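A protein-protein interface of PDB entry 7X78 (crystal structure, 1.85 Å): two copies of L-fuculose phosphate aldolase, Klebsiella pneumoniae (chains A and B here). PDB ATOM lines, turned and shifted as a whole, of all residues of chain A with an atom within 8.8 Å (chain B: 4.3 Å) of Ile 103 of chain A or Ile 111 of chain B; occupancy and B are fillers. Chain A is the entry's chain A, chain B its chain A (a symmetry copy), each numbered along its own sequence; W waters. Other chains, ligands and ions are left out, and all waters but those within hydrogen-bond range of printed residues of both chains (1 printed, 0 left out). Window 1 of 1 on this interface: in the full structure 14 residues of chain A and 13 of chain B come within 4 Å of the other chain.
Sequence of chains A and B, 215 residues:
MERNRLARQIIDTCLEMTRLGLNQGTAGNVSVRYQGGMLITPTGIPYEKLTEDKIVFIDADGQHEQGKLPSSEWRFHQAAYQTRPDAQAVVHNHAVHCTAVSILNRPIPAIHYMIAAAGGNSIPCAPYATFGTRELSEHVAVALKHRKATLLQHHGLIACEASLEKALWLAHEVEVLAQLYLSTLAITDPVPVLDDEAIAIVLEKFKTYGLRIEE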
ATOM      1  N   ALA A  95      22.238   0.482  25.425  1.00  0.00           N
ATOM      2  CA  ALA A  95      22.203   0.177  23.999  1.00  0.00           C
ATOM      3  C   ALA A  95      23.425   0.785  23.317  1.00  0.00           C
ATOM      4  O   ALA A  95      23.840   1.899  23.632  1.00  0.00           O
ATOM      5  CB  ALA A  95      20.909   0.720  23.385  1.00  0.00           C
ATOM      6  N   VAL A  96      24.022   0.034  22.396  1.00  0.00           N
ATOM      7  CA  VAL A  96      25.387   0.348  21.990  1.00  0.00           C
ATOM      8  C   VAL A  96      25.463   1.682  21.238  1.00  0.00           C
ATOM      9  O   VAL A  96      26.385   2.479  21.458  1.00  0.00           O
ATOM     10  CB  VAL A  96      25.966  -0.834  21.186  1.00  0.00           C
ATOM     11  CG1 VAL A  96      25.278  -0.971  19.837  1.00  0.00           C
ATOM     12  CG2 VAL A  96      27.465  -0.687  21.032  1.00  0.00           C
ATOM     13  N   HIS A  97      24.501   1.976  20.356  1.00  0.00           N
ATOM     14  CA  HIS A  97      24.604   3.228  19.604  1.00  0.00           C
ATOM     15  C   HIS A  97      24.314   4.432  20.498  1.00  0.00           C
ATOM     16  O   HIS A  97      25.059   5.421  20.476  1.00  0.00           O
ATOM     17  CB  HIS A  97      23.681   3.178  18.379  1.00  0.00           C
ATOM     18  CG  HIS A  97      24.029   2.063  17.442  1.00  0.00           C
ATOM     19  ND1 HIS A  97      23.346   0.866  17.423  1.00  0.00           N
ATOM     20  CD2 HIS A  97      25.027   1.940  16.534  1.00  0.00           C
ATOM     21  CE1 HIS A  97      23.895   0.062  16.530  1.00  0.00           C
ATOM     22  NE2 HIS A  97      24.916   0.692  15.974  1.00  0.00           N
ATOM     23  N   CYS A  98      23.253   4.355  21.309  1.00  0.00           N
ATOM     24  CA  CYS A  98      22.979   5.377  22.325  1.00  0.00           C
ATOM     25  C   CYS A  98      24.211   5.641  23.176  1.00  0.00           C
ATOM     26  O   CYS A  98      24.589   6.791  23.444  1.00  0.00           O
ATOM     27  CB  CYS A  98      21.846   4.900  23.242  1.00  0.00           C
ATOM     28  SG  CYS A  98      20.219   5.084  22.569  1.00  0.00           S
ATOM     29  N   THR A  99      24.837   4.569  23.634  1.00  0.00           N
ATOM     30  CA  THR A  99      25.931   4.703  24.584  1.00  0.00           C
ATOM     31  C   THR A  99      27.164   5.304  23.917  1.00  0.00           C
ATOM     32  O   THR A  99      27.852   6.139  24.514  1.00  0.00           O
ATOM     33  CB  THR A  99      26.200   3.333  25.211  1.00  0.00           C
ATOM     34  OG1 THR A  99      24.988   2.899  25.864  1.00  0.00           O
ATOM     35  CG2 THR A  99      27.338   3.389  26.226  1.00  0.00           C
ATOM     36  N   ALA A 100      27.428   4.927  22.664  1.00  0.00           N
ATOM     37  CA  ALA A 100      28.525   5.544  21.924  1.00  0.00           C
ATOM     38  C   ALA A 100      28.326   7.046  21.768  1.00  0.00           C
ATOM     39  O   ALA A 100      29.277   7.818  21.950  1.00  0.00           O
ATOM     40  CB  ALA A 100      28.691   4.889  20.548  1.00  0.00           C
ATOM     41  N   VAL A 101      27.109   7.486  21.424  1.00  0.00           N
ATOM     42  CA  VAL A 101      26.865   8.929  21.354  1.00  0.00           C
ATOM     43  C   VAL A 101      27.099   9.569  22.718  1.00  0.00           C
ATOM     44  O   VAL A 101      27.673  10.660  22.817  1.00  0.00           O
ATOM     45  CB  VAL A 101      25.450   9.230  20.834  1.00  0.00           C
ATOM     46  CG1 VAL A 101      25.155  10.748  20.950  1.00  0.00           C
ATOM     47  CG2 VAL A 101      25.308   8.770  19.372  1.00  0.00           C
ATOM     48  N   SER A 102      26.664   8.901  23.789  1.00  0.00           N
ATOM     49  CA  SER A 102      26.845   9.449  25.134  1.00  0.00           C
ATOM     50  C   SER A 102      28.316   9.514  25.532  1.00  0.00           C
ATOM     51  O   SER A 102      28.697  10.355  26.357  1.00  0.00           O
ATOM     52  CB  SER A 102      26.051   8.620  26.151  1.00  0.00           C
ATOM     53  OG  SER A 102      26.863   7.561  26.635  1.00  0.00           O
ATOM     54  N   ILE A 103      29.160   8.658  24.953  1.00  0.00           N
ATOM     55  CA  ILE A 103      30.593   8.755  25.220  1.00  0.00           C
ATOM     56  C   ILE A 103      31.186  10.016  24.603  1.00  0.00           C
ATOM     57  O   ILE A 103      32.124  10.606  25.156  1.00  0.00           O
ATOM     58  CB  ILE A 103      31.297   7.482  24.722  1.00  0.00           C
ATOM     59  CG1 ILE A 103      30.943   6.317  25.649  1.00  0.00           C
ATOM     60  CG2 ILE A 103      32.815   7.663  24.651  1.00  0.00           C
ATOM     61  CD1 ILE A 103      31.432   4.959  25.143  1.00  0.00           C
ATOM     62  N   LEU A 104      30.655  10.455  23.468  1.00  0.00           N
ATOM     63  CA  LEU A 104      31.089  11.712  22.879  1.00  0.00           C
ATOM     64  C   LEU A 104      30.504  12.926  23.591  1.00  0.00           C
ATOM     65  O   LEU A 104      30.906  14.056  23.283  1.00  0.00           O
ATOM     66  CB  LEU A 104      30.696  11.756  21.403  1.00  0.00           C
ATOM     67  CG  LEU A 104      31.130  10.598  20.509  1.00  0.00           C
ATOM     68  CD1 LEU A 104      30.459  10.690  19.157  1.00  0.00           C
ATOM     69  CD2 LEU A 104      32.635  10.577  20.355  1.00  0.00           C
ATOM     70  N   ASN A 105      29.569  12.715  24.521  1.00  0.00           N
ATOM     71  CA  ASN A 105      28.883  13.792  25.241  1.00  0.00           C
ATOM     72  C   ASN A 105      28.235  14.764  24.258  1.00  0.00           C
ATOM     73  O   ASN A 105      28.425  15.980  24.321  1.00  0.00           O
ATOM     74  CB  ASN A 105      29.829  14.520  26.208  1.00  0.00           C
ATOM     75  CG  ASN A 105      29.081  15.381  27.217  1.00  0.00           C
ATOM     76  OD1 ASN A 105      27.923  15.130  27.524  1.00  0.00           O
ATOM     77  ND2 ASN A 105      29.750  16.396  27.740  1.00  0.00           N
ATOM     78  N   ARG A 106      27.472  14.208  23.325  1.00  0.00           N
ATOM     79  CA  ARG A 106      26.743  15.001  22.354  1.00  0.00           C
ATOM     80  C   ARG A 106      25.258  14.705  22.466  1.00  0.00           C
ATOM     81  O   ARG A 106      24.875  13.540  22.609  1.00  0.00           O
ATOM     82  CB  ARG A 106      27.190  14.683  20.914  1.00  0.00           C
ATOM     83  CG  ARG A 106      28.570  15.165  20.511  1.00  0.00           C
ATOM     84  CD  ARG A 106      28.889  14.560  19.152  1.00  0.00           C
ATOM     85  NE  ARG A 106      30.154  14.998  18.574  1.00  0.00           N
ATOM     86  CZ  ARG A 106      30.248  15.648  17.420  1.00  0.00           C
ATOM     87  NH1 ARG A 106      29.148  15.939  16.738  1.00  0.00           N
ATOM     88  NH2 ARG A 106      31.435  16.008  16.950  1.00  0.00           N
ATOM     89  N   CYS A 125      22.009  14.966  26.304  1.00  0.00           N
ATOM     90  CA  CYS A 125      23.038  14.122  26.906  1.00  0.00           C
ATOM     91  C   CYS A 125      23.423  14.755  28.231  1.00  0.00           C
ATOM     92  O   CYS A 125      24.133  15.767  28.249  1.00  0.00           O
ATOM     93  CB  CYS A 125      24.260  13.972  25.997  1.00  0.00           C
ATOM     94  SG  CYS A 125      25.454  12.756  26.639  1.00  0.00           S
ATOM     95  N   ALA A 126      22.969  14.146  29.327  1.00  0.00           N
ATOM     96  CA  ALA A 126      23.237  14.679  30.655  1.00  0.00           C
ATOM     97  C   ALA A 126      24.689  14.427  31.057  1.00  0.00           C
ATOM     98  O   ALA A 126      25.250  13.376  30.726  1.00  0.00           O
ATOM     99  CB  ALA A 126      22.293  14.046  31.691  1.00  0.00           C
ATOM    100  N   TYR A 128      28.097  13.386  33.078  1.00  0.00           N
ATOM    101  CA  TYR A 128      28.431  12.185  33.855  1.00  0.00           C
ATOM    102  C   TYR A 128      28.369  12.428  35.361  1.00  0.00           C
ATOM    103  O   TYR A 128      28.758  13.486  35.861  1.00  0.00           O
ATOM    104  CB  TYR A 128      29.852  11.677  33.508  1.00  0.00           C
ATOM    105  CG  TYR A 128      30.260  10.447  34.325  1.00  0.00           C
ATOM    106  CD1 TYR A 128      29.844   9.176  33.945  1.00  0.00           C
ATOM    107  CD2 TYR A 128      31.034  10.563  35.484  1.00  0.00           C
ATOM    108  CE1 TYR A 128      30.184   8.043  34.693  1.00  0.00           C
ATOM    109  CE2 TYR A 128      31.387   9.431  36.240  1.00  0.00           C
ATOM    110  CZ  TYR A 128      30.953   8.177  35.829  1.00  0.00           C
ATOM    111  OH  TYR A 128      31.271   7.047  36.545  1.00  0.00           O
ATOM    112  N   LEU A 151      20.118  10.765  26.943  1.00  0.00           N
ATOM    113  CA  LEU A 151      21.359  10.047  27.118  1.00  0.00           C
ATOM    114  C   LEU A 151      22.014  10.458  28.427  1.00  0.00           C
ATOM    115  O   LEU A 151      21.753  11.533  28.972  1.00  0.00           O
ATOM    116  CB  LEU A 151      22.324  10.312  25.967  1.00  0.00           C
ATOM    117  CG  LEU A 151      21.736  10.030  24.590  1.00  0.00           C
ATOM    118  CD1 LEU A 151      22.781  10.349  23.558  1.00  0.00           C
ATOM    119  CD2 LEU A 151      21.261   8.580  24.470  1.00  0.00           C
ATOM    120  N   LEU A 152      22.891   9.576  28.909  1.00  0.00           N
ATOM    121  CA  LEU A 152      23.700   9.777  30.107  1.00  0.00           C
ATOM    122  C   LEU A 152      25.155   9.628  29.705  1.00  0.00           C
ATOM    123  O   LEU A 152      25.555   8.546  29.268  1.00  0.00           O
ATOM    124  CB  LEU A 152      23.370   8.738  31.183  1.00  0.00           C
ATOM    125  CG  LEU A 152      21.911   8.437  31.498  1.00  0.00           C
ATOM    126  CD1 LEU A 152      21.825   7.275  32.490  1.00  0.00           C
ATOM    127  CD2 LEU A 152      21.286   9.688  32.067  1.00  0.00           C
ATOM    128  N   GLN A 153      25.942  10.694  29.864  1.00  0.00           N
ATOM    129  CA  GLN A 153      27.322  10.686  29.389  1.00  0.00           C
ATOM    130  C   GLN A 153      28.104   9.491  29.944  1.00  0.00           C
ATOM    131  O   GLN A 153      28.042   9.197  31.138  1.00  0.00           O
ATOM    132  CB  GLN A 153      28.005  12.004  29.778  1.00  0.00           C
ATOM    133  CG  GLN A 153      29.466  12.110  29.342  1.00  0.00           C
ATOM    134  CD  GLN A 153      30.157  13.340  29.894  1.00  0.00           C
ATOM    135  OE1 GLN A 153      29.673  13.974  30.831  1.00  0.00           O
ATOM    136  NE2 GLN A 153      31.312  13.682  29.318  1.00  0.00           N
ATOM    137  N   HIS A 154      28.838   8.799  29.058  1.00  0.00           N
ATOM    138  CA  HIS A 154      29.649   7.628  29.416  1.00  0.00           C
ATOM    139  C   HIS A 154      28.822   6.502  30.026  1.00  0.00           C
ATOM    140  O   HIS A 154      29.342   5.692  30.796  1.00  0.00           O
ATOM    141  CB  HIS A 154      30.779   7.994  30.382  1.00  0.00           C
ATOM    142  CG  HIS A 154      31.928   8.695  29.730  1.00  0.00           C
ATOM    143  ND1 HIS A 154      32.745   8.085  28.798  1.00  0.00           N
ATOM    144  CD2 HIS A 154      32.410   9.951  29.889  1.00  0.00           C
ATOM    145  CE1 HIS A 154      33.681   8.937  28.410  1.00  0.00           C
ATOM    146  NE2 HIS A 154      33.500  10.077  29.057  1.00  0.00           N
ATOM    147  N   HIS A 155      27.550   6.405  29.674  1.00  0.00           N
ATOM    148  CA  HIS A 155      26.685   5.497  30.415  1.00  0.00           C
ATOM    149  C   HIS A 155      25.676   4.786  29.525  1.00  0.00           C
ATOM    150  O   HIS A 155      25.789   3.571  29.301  1.00  0.00           O
ATOM    151  CB  HIS A 155      25.966   6.269  31.518  1.00  0.00           C
ATOM    152  CG  HIS A 155      25.293   5.388  32.525  1.00  0.00           C
ATOM    153  ND1 HIS A 155      25.360   5.626  33.880  1.00  0.00           N
ATOM    154  CD2 HIS A 155      24.549   4.266  32.375  1.00  0.00           C
ATOM    155  CE1 HIS A 155      24.680   4.692  34.522  1.00  0.00           C
ATOM    156  NE2 HIS A 155      24.177   3.854  33.632  1.00  0.00           N
ATOM    157  N   GLY A 156      24.686   5.524  29.024  1.00  0.00           N
ATOM    158  CA  GLY A 156      23.617   4.930  28.237  1.00  0.00           C
ATOM    159  C   GLY A 156      22.393   5.809  28.096  1.00  0.00           C
ATOM    160  O   GLY A 156      22.514   7.019  27.890  1.00  0.00           O
ATOM    161  N   LEU A 182      25.441   8.328  14.396  1.00  0.00           N
ATOM    162  CA  LEU A 182      26.804   7.807  14.262  1.00  0.00           C
ATOM    163  C   LEU A 182      27.152   7.517  12.809  1.00  0.00           C
ATOM    164  O   LEU A 182      28.273   7.802  12.359  1.00  0.00           O
ATOM    165  CB  LEU A 182      26.979   6.536  15.093  1.00  0.00           C
ATOM    166  CG  LEU A 182      26.877   6.781  16.604  1.00  0.00           C
ATOM    167  CD1 LEU A 182      26.678   5.460  17.319  1.00  0.00           C
ATOM    168  CD2 LEU A 182      28.110   7.537  17.133  1.00  0.00           C
ATOM    169  N   PRO B 109      40.502   1.760  26.421  1.00  0.00           N
ATOM    170  CA  PRO B 109      40.619   2.618  27.611  1.00  0.00           C
ATOM    171  C   PRO B 109      39.284   2.821  28.319  1.00  0.00           C
ATOM    172  O   PRO B 109      38.268   2.222  27.948  1.00  0.00           O
ATOM    173  CB  PRO B 109      41.180   3.925  27.037  1.00  0.00           C
ATOM    174  CG  PRO B 109      40.598   3.987  25.635  1.00  0.00           C
ATOM    175  CD  PRO B 109      40.416   2.537  25.171  1.00  0.00           C
ATOM    176  N   ALA B 110      39.266   3.690  29.329  1.00  0.00           N
ATOM    177  CA  ALA B 110      38.113   3.825  30.218  1.00  0.00           C
ATOM    178  C   ALA B 110      37.002   4.681  29.594  1.00  0.00           C
ATOM    179  O   ALA B 110      36.575   5.694  30.138  1.00  0.00           O
ATOM    180  CB  ALA B 110      38.570   4.393  31.556  1.00  0.00           C
ATOM    181  N   ILE B 111      36.487   4.225  28.445  1.00  0.00           N
ATOM    182  CA  ILE B 111      35.439   4.976  27.748  1.00  0.00           C
ATOM    183  C   ILE B 111      34.067   4.775  28.368  1.00  0.00           C
ATOM    184  O   ILE B 111      33.136   5.534  28.067  1.00  0.00           O
ATOM    185  CB  ILE B 111      35.385   4.590  26.257  1.00  0.00           C
ATOM    186  CG1 ILE B 111      35.046   3.099  26.107  1.00  0.00           C
ATOM    187  CG2 ILE B 111      36.727   4.906  25.592  1.00  0.00           C
ATOM    188  CD1 ILE B 111      34.892   2.644  24.668  1.00  0.00           C
ATOM    189  N   HIS B 112      33.921   3.796  29.251  1.00  0.00           N
ATOM    190  CA  HIS B 112      32.627   3.469  29.836  1.00  0.00           C
ATOM    191  C   HIS B 112      32.893   2.805  31.179  1.00  0.00           C
ATOM    192  O   HIS B 112      33.864   2.062  31.309  1.00  0.00           O
ATOM    193  CB  HIS B 112      31.833   2.539  28.915  1.00  0.00           C
ATOM    194  CG  HIS B 112      30.431   2.298  29.372  1.00  0.00           C
ATOM    195  ND1 HIS B 112      30.110   1.378  30.344  1.00  0.00           N
ATOM    196  CD2 HIS B 112      29.263   2.872  28.995  1.00  0.00           C
ATOM    197  CE1 HIS B 112      28.805   1.391  30.543  1.00  0.00           C
ATOM    198  NE2 HIS B 112      28.268   2.288  29.735  1.00  0.00           N
ATOM    199  N   LEU B 177      32.152  -3.111  24.789  1.00  0.00           N
ATOM    200  CA  LEU B 177      33.146  -2.057  24.962  1.00  0.00           C
ATOM    201  C   LEU B 177      33.957  -1.842  23.691  1.00  0.00           C
ATOM    202  O   LEU B 177      34.251  -0.700  23.316  1.00  0.00           O
ATOM    203  CB  LEU B 177      34.078  -2.406  26.120  1.00  0.00           C
ATOM    204  CG  LEU B 177      33.456  -2.300  27.508  1.00  0.00           C
ATOM    205  CD1 LEU B 177      34.409  -2.899  28.549  1.00  0.00           C
ATOM    206  CD2 LEU B 177      33.154  -0.841  27.825  1.00  0.00           C
ATOM    207  N   LEU B 180      31.895  -0.054  21.170  1.00  0.00           N
ATOM    208  CA  LEU B 180      31.786   1.346  21.575  1.00  0.00           C
ATOM    209  C   LEU B 180      33.032   2.121  21.175  1.00  0.00           C
ATOM    210  O   LEU B 180      32.954   3.222  20.617  1.00  0.00           O
ATOM    211  CB  LEU B 180      31.573   1.426  23.086  1.00  0.00           C
ATOM    212  CG  LEU B 180      30.214   0.990  23.633  1.00  0.00           C
ATOM    213  CD1 LEU B 180      30.258   0.878  25.158  1.00  0.00           C
ATOM    214  CD2 LEU B 180      29.122   1.967  23.194  1.00  0.00           C
ATOM    215  N   TYR B 181      34.192   1.539  21.454  1.00  0.00           N
ATOM    216  CA  TYR B 181      35.464   2.169  21.125  1.00  0.00           C
ATOM    217  C   TYR B 181      35.613   2.374  19.621  1.00  0.00           C
ATOM    218  O   TYR B 181      35.969   3.469  19.174  1.00  0.00           O
ATOM    219  CB  TYR B 181      36.594   1.316  21.693  1.00  0.00           C
ATOM    220  CG  TYR B 181      37.924   2.012  21.716  1.00  0.00           C
ATOM    221  CD1 TYR B 181      38.010   3.384  21.931  1.00  0.00           C
ATOM    222  CD2 TYR B 181      39.099   1.296  21.521  1.00  0.00           C
ATOM    223  CE1 TYR B 181      39.242   4.027  21.934  1.00  0.00           C
ATOM    224  CE2 TYR B 181      40.332   1.931  21.530  1.00  0.00           C
ATOM    225  CZ  TYR B 181      40.395   3.290  21.733  1.00  0.00           C
ATOM    226  OH  TYR B 181      41.636   3.910  21.736  1.00  0.00           O
ATOM    227  N   THR B 184      33.194   5.196  18.373  1.00  0.00           N
ATOM    228  CA  THR B 184      33.582   6.551  18.739  1.00  0.00           C
ATOM    229  C   THR B 184      34.917   6.936  18.111  1.00  0.00           C
ATOM    230  O   THR B 184      35.093   8.085  17.685  1.00  0.00           O
ATOM    231  CB  THR B 184      33.633   6.703  20.264  1.00  0.00           C
ATOM    232  OG1 THR B 184      34.395   5.645  20.860  1.00  0.00           O
ATOM    233  CG2 THR B 184      32.218   6.681  20.849  1.00  0.00           C
ATOM    234  N   VAL B 191      39.347   9.057  21.976  1.00  0.00           N
ATOM    235  CA  VAL B 191      38.004   9.024  22.549  1.00  0.00           C
ATOM    236  C   VAL B 191      38.044   9.540  23.986  1.00  0.00           C
ATOM    237  O   VAL B 191      38.975   9.204  24.733  1.00  0.00           O
ATOM    238  CB  VAL B 191      37.426   7.602  22.488  1.00  0.00           C
ATOM    239  CG1 VAL B 191      36.054   7.567  23.153  1.00  0.00           C
ATOM    240  CG2 VAL B 191      37.321   7.145  21.023  1.00  0.00           C
ATOM    241  N   PRO B 192      37.074  10.353  24.409  1.00  0.00           N
ATOM    242  CA  PRO B 192      37.028  10.783  25.815  1.00  0.00           C
ATOM    243  C   PRO B 192      36.977   9.593  26.762  1.00  0.00           C
ATOM    244  O   PRO B 192      36.315   8.592  26.495  1.00  0.00           O
ATOM    245  CB  PRO B 192      35.739  11.611  25.893  1.00  0.00           C
ATOM    246  CG  PRO B 192      35.479  12.067  24.488  1.00  0.00           C
ATOM    247  CD  PRO B 192      36.045  11.009  23.580  1.00  0.00           C
ATOM    248  N   VAL B 193      37.676   9.712  27.890  1.00  0.00           N
ATOM    249  CA  VAL B 193      37.672   8.658  28.894  1.00  0.00           C
ATOM    250  C   VAL B 193      37.324   9.232  30.258  1.00  0.00           C
ATOM    251  O   VAL B 193      37.476  10.429  30.525  1.00  0.00           O
ATOM    252  CB  VAL B 193      39.019   7.893  28.977  1.00  0.00           C
ATOM    253  CG1 VAL B 193      39.350   7.256  27.640  1.00  0.00           C
ATOM    254  CG2 VAL B 193      40.143   8.812  29.448  1.00  0.00           C
HETATM  255  O   HOH W   1      35.175  12.080  29.764  1.00  0.00           O
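Water W1 bridges NE2 of His 154 of chain A and O of Val 193 of chain B.
Among the printed residues, merely in contact across the chains: Val 96 of chain A with Leu 180 of chain B (3.3 Å), Thr 99 of chain A with His 112 of chain B (3.4 Å), Thr 99 of chain A with Leu 180 of chain B (3.8 Å), Ala 100 of chain A with Leu 180 of chain B (3.5 Å), Ala 100 of chain A with Thr 184 of chain B (3.3 Å), Ile 103 of chain A with Ile 111 of chain B (3.4 Å), Ile 103 of chain A with Thr 184 of chain B (3.97 Å), Ile 103 of chain A with Val 191 of chain B (3.6 Å), Ile 103 of chain A with Pro 192 of chain B (3.7 Å), Leu 104 of chain A with Thr 184 of chain B (3.9 Å), His 154 of chain A with His 112 of chain B (3.3 Å) and His 154 of chain A with Pro 192 of chain B (3.3 Å).
Of the printed residues of chain B, Thr 99 of chain A touches His 112 (3.4 Å) and Leu 180 (3.8 Å).
Of chain B, only Ile 111, Thr 184, Val 191 and Pro 192 come within 4 Å of Ile 103 of chain A.
Of the printed residues of chain B, His 154 of chain A touches Ile 111, His 112 and Pro 192.
Of the printed residues of chain B, His 155 of chain A touches His 112.
Leu 182 of chain A touches none of the printed residues of chain B.
No residue of chain A comes within 4 Å of Ala 110 of chain B.
Of chain A, only Ile 103 and His 154 come within 4 Å of Ile 111 of chain B.
Tyr 181 of chain B touches none of the printed residues of chain A.
Of the printed residues of chain A, Val 191 of chain B touches Ile 103 (3.6 Å).
Printed residues of chain A within 4 Å of Pro 192 of chain B: Ile 103 and His 154.
The nearest residue of chain A that does not touch Ile 111 of chain B is His 155 of chain A (5.9 Å).
The nearest printed residue of chain B that does not touch Ala 100 of chain A is Tyr 181 of chain B (6.5 Å).
The backbone carbonyl oxygen (O) of Ile 111 of chain B lies within hydrogen-bond range of a ring nitrogen (ND1) of His 154 of chain A (2.7 Å).
The backbone carbonyl oxygen of His 155 of chain A lies within hydrogen-bond range of a ring nitrogen (NE2) of His 112 of chain B, at 2.8 Å.
Along chain A the printed residues that touch a printed residue of chain B span positions 96 to 155.
Printed residues of chain B that touch a printed residue of chain A: Ile 111, His 112, Leu 180, Thr 184, Val 191 and Pro 192.
Hydrophobic or aromatic side chains of chain B that line the printed part of chain A: His 112, Leu 180, Val 191 and Pro 192.
Among the printed residues, no Asp or Glu carboxylate lies within 4 Å of a Lys or Arg side-chain nitrogen of the other chain.
OG of Ser 102 of chain A is in hydrogen-bond range of N of His 155 of chain A, at 3.3 Å.
OG1 of Thr 184 of chain B is in hydrogen-bond range of O of Tyr 181 of chain B.
O of Ala 95 of chain A is in hydrogen-bond range of OG1 of Thr 99 of chain A (2.7 Å).
The backbone NH of His 154 of chain A is in hydrogen-bond range of the backbone carbonyl oxygen of Ser 102 of chain A (3.1 Å).
The backbone carbonyl oxygen (O) of Thr 99 of chain A sits at hydrogen-bond distance from the side-chain hydroxyl (OG) of Ser 102 of chain A (2.7 Å).
The side-chain hydroxyl (OG1) of Thr 184 of chain B is in hydrogen-bond range of the backbone carbonyl oxygen (O) of Leu 180 of chain B (2.8 Å).
No position is printed for both chains.
Of the 14 pairs that touch across the chains among the printed residues, none has its exchanged pair printed and touching as well.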
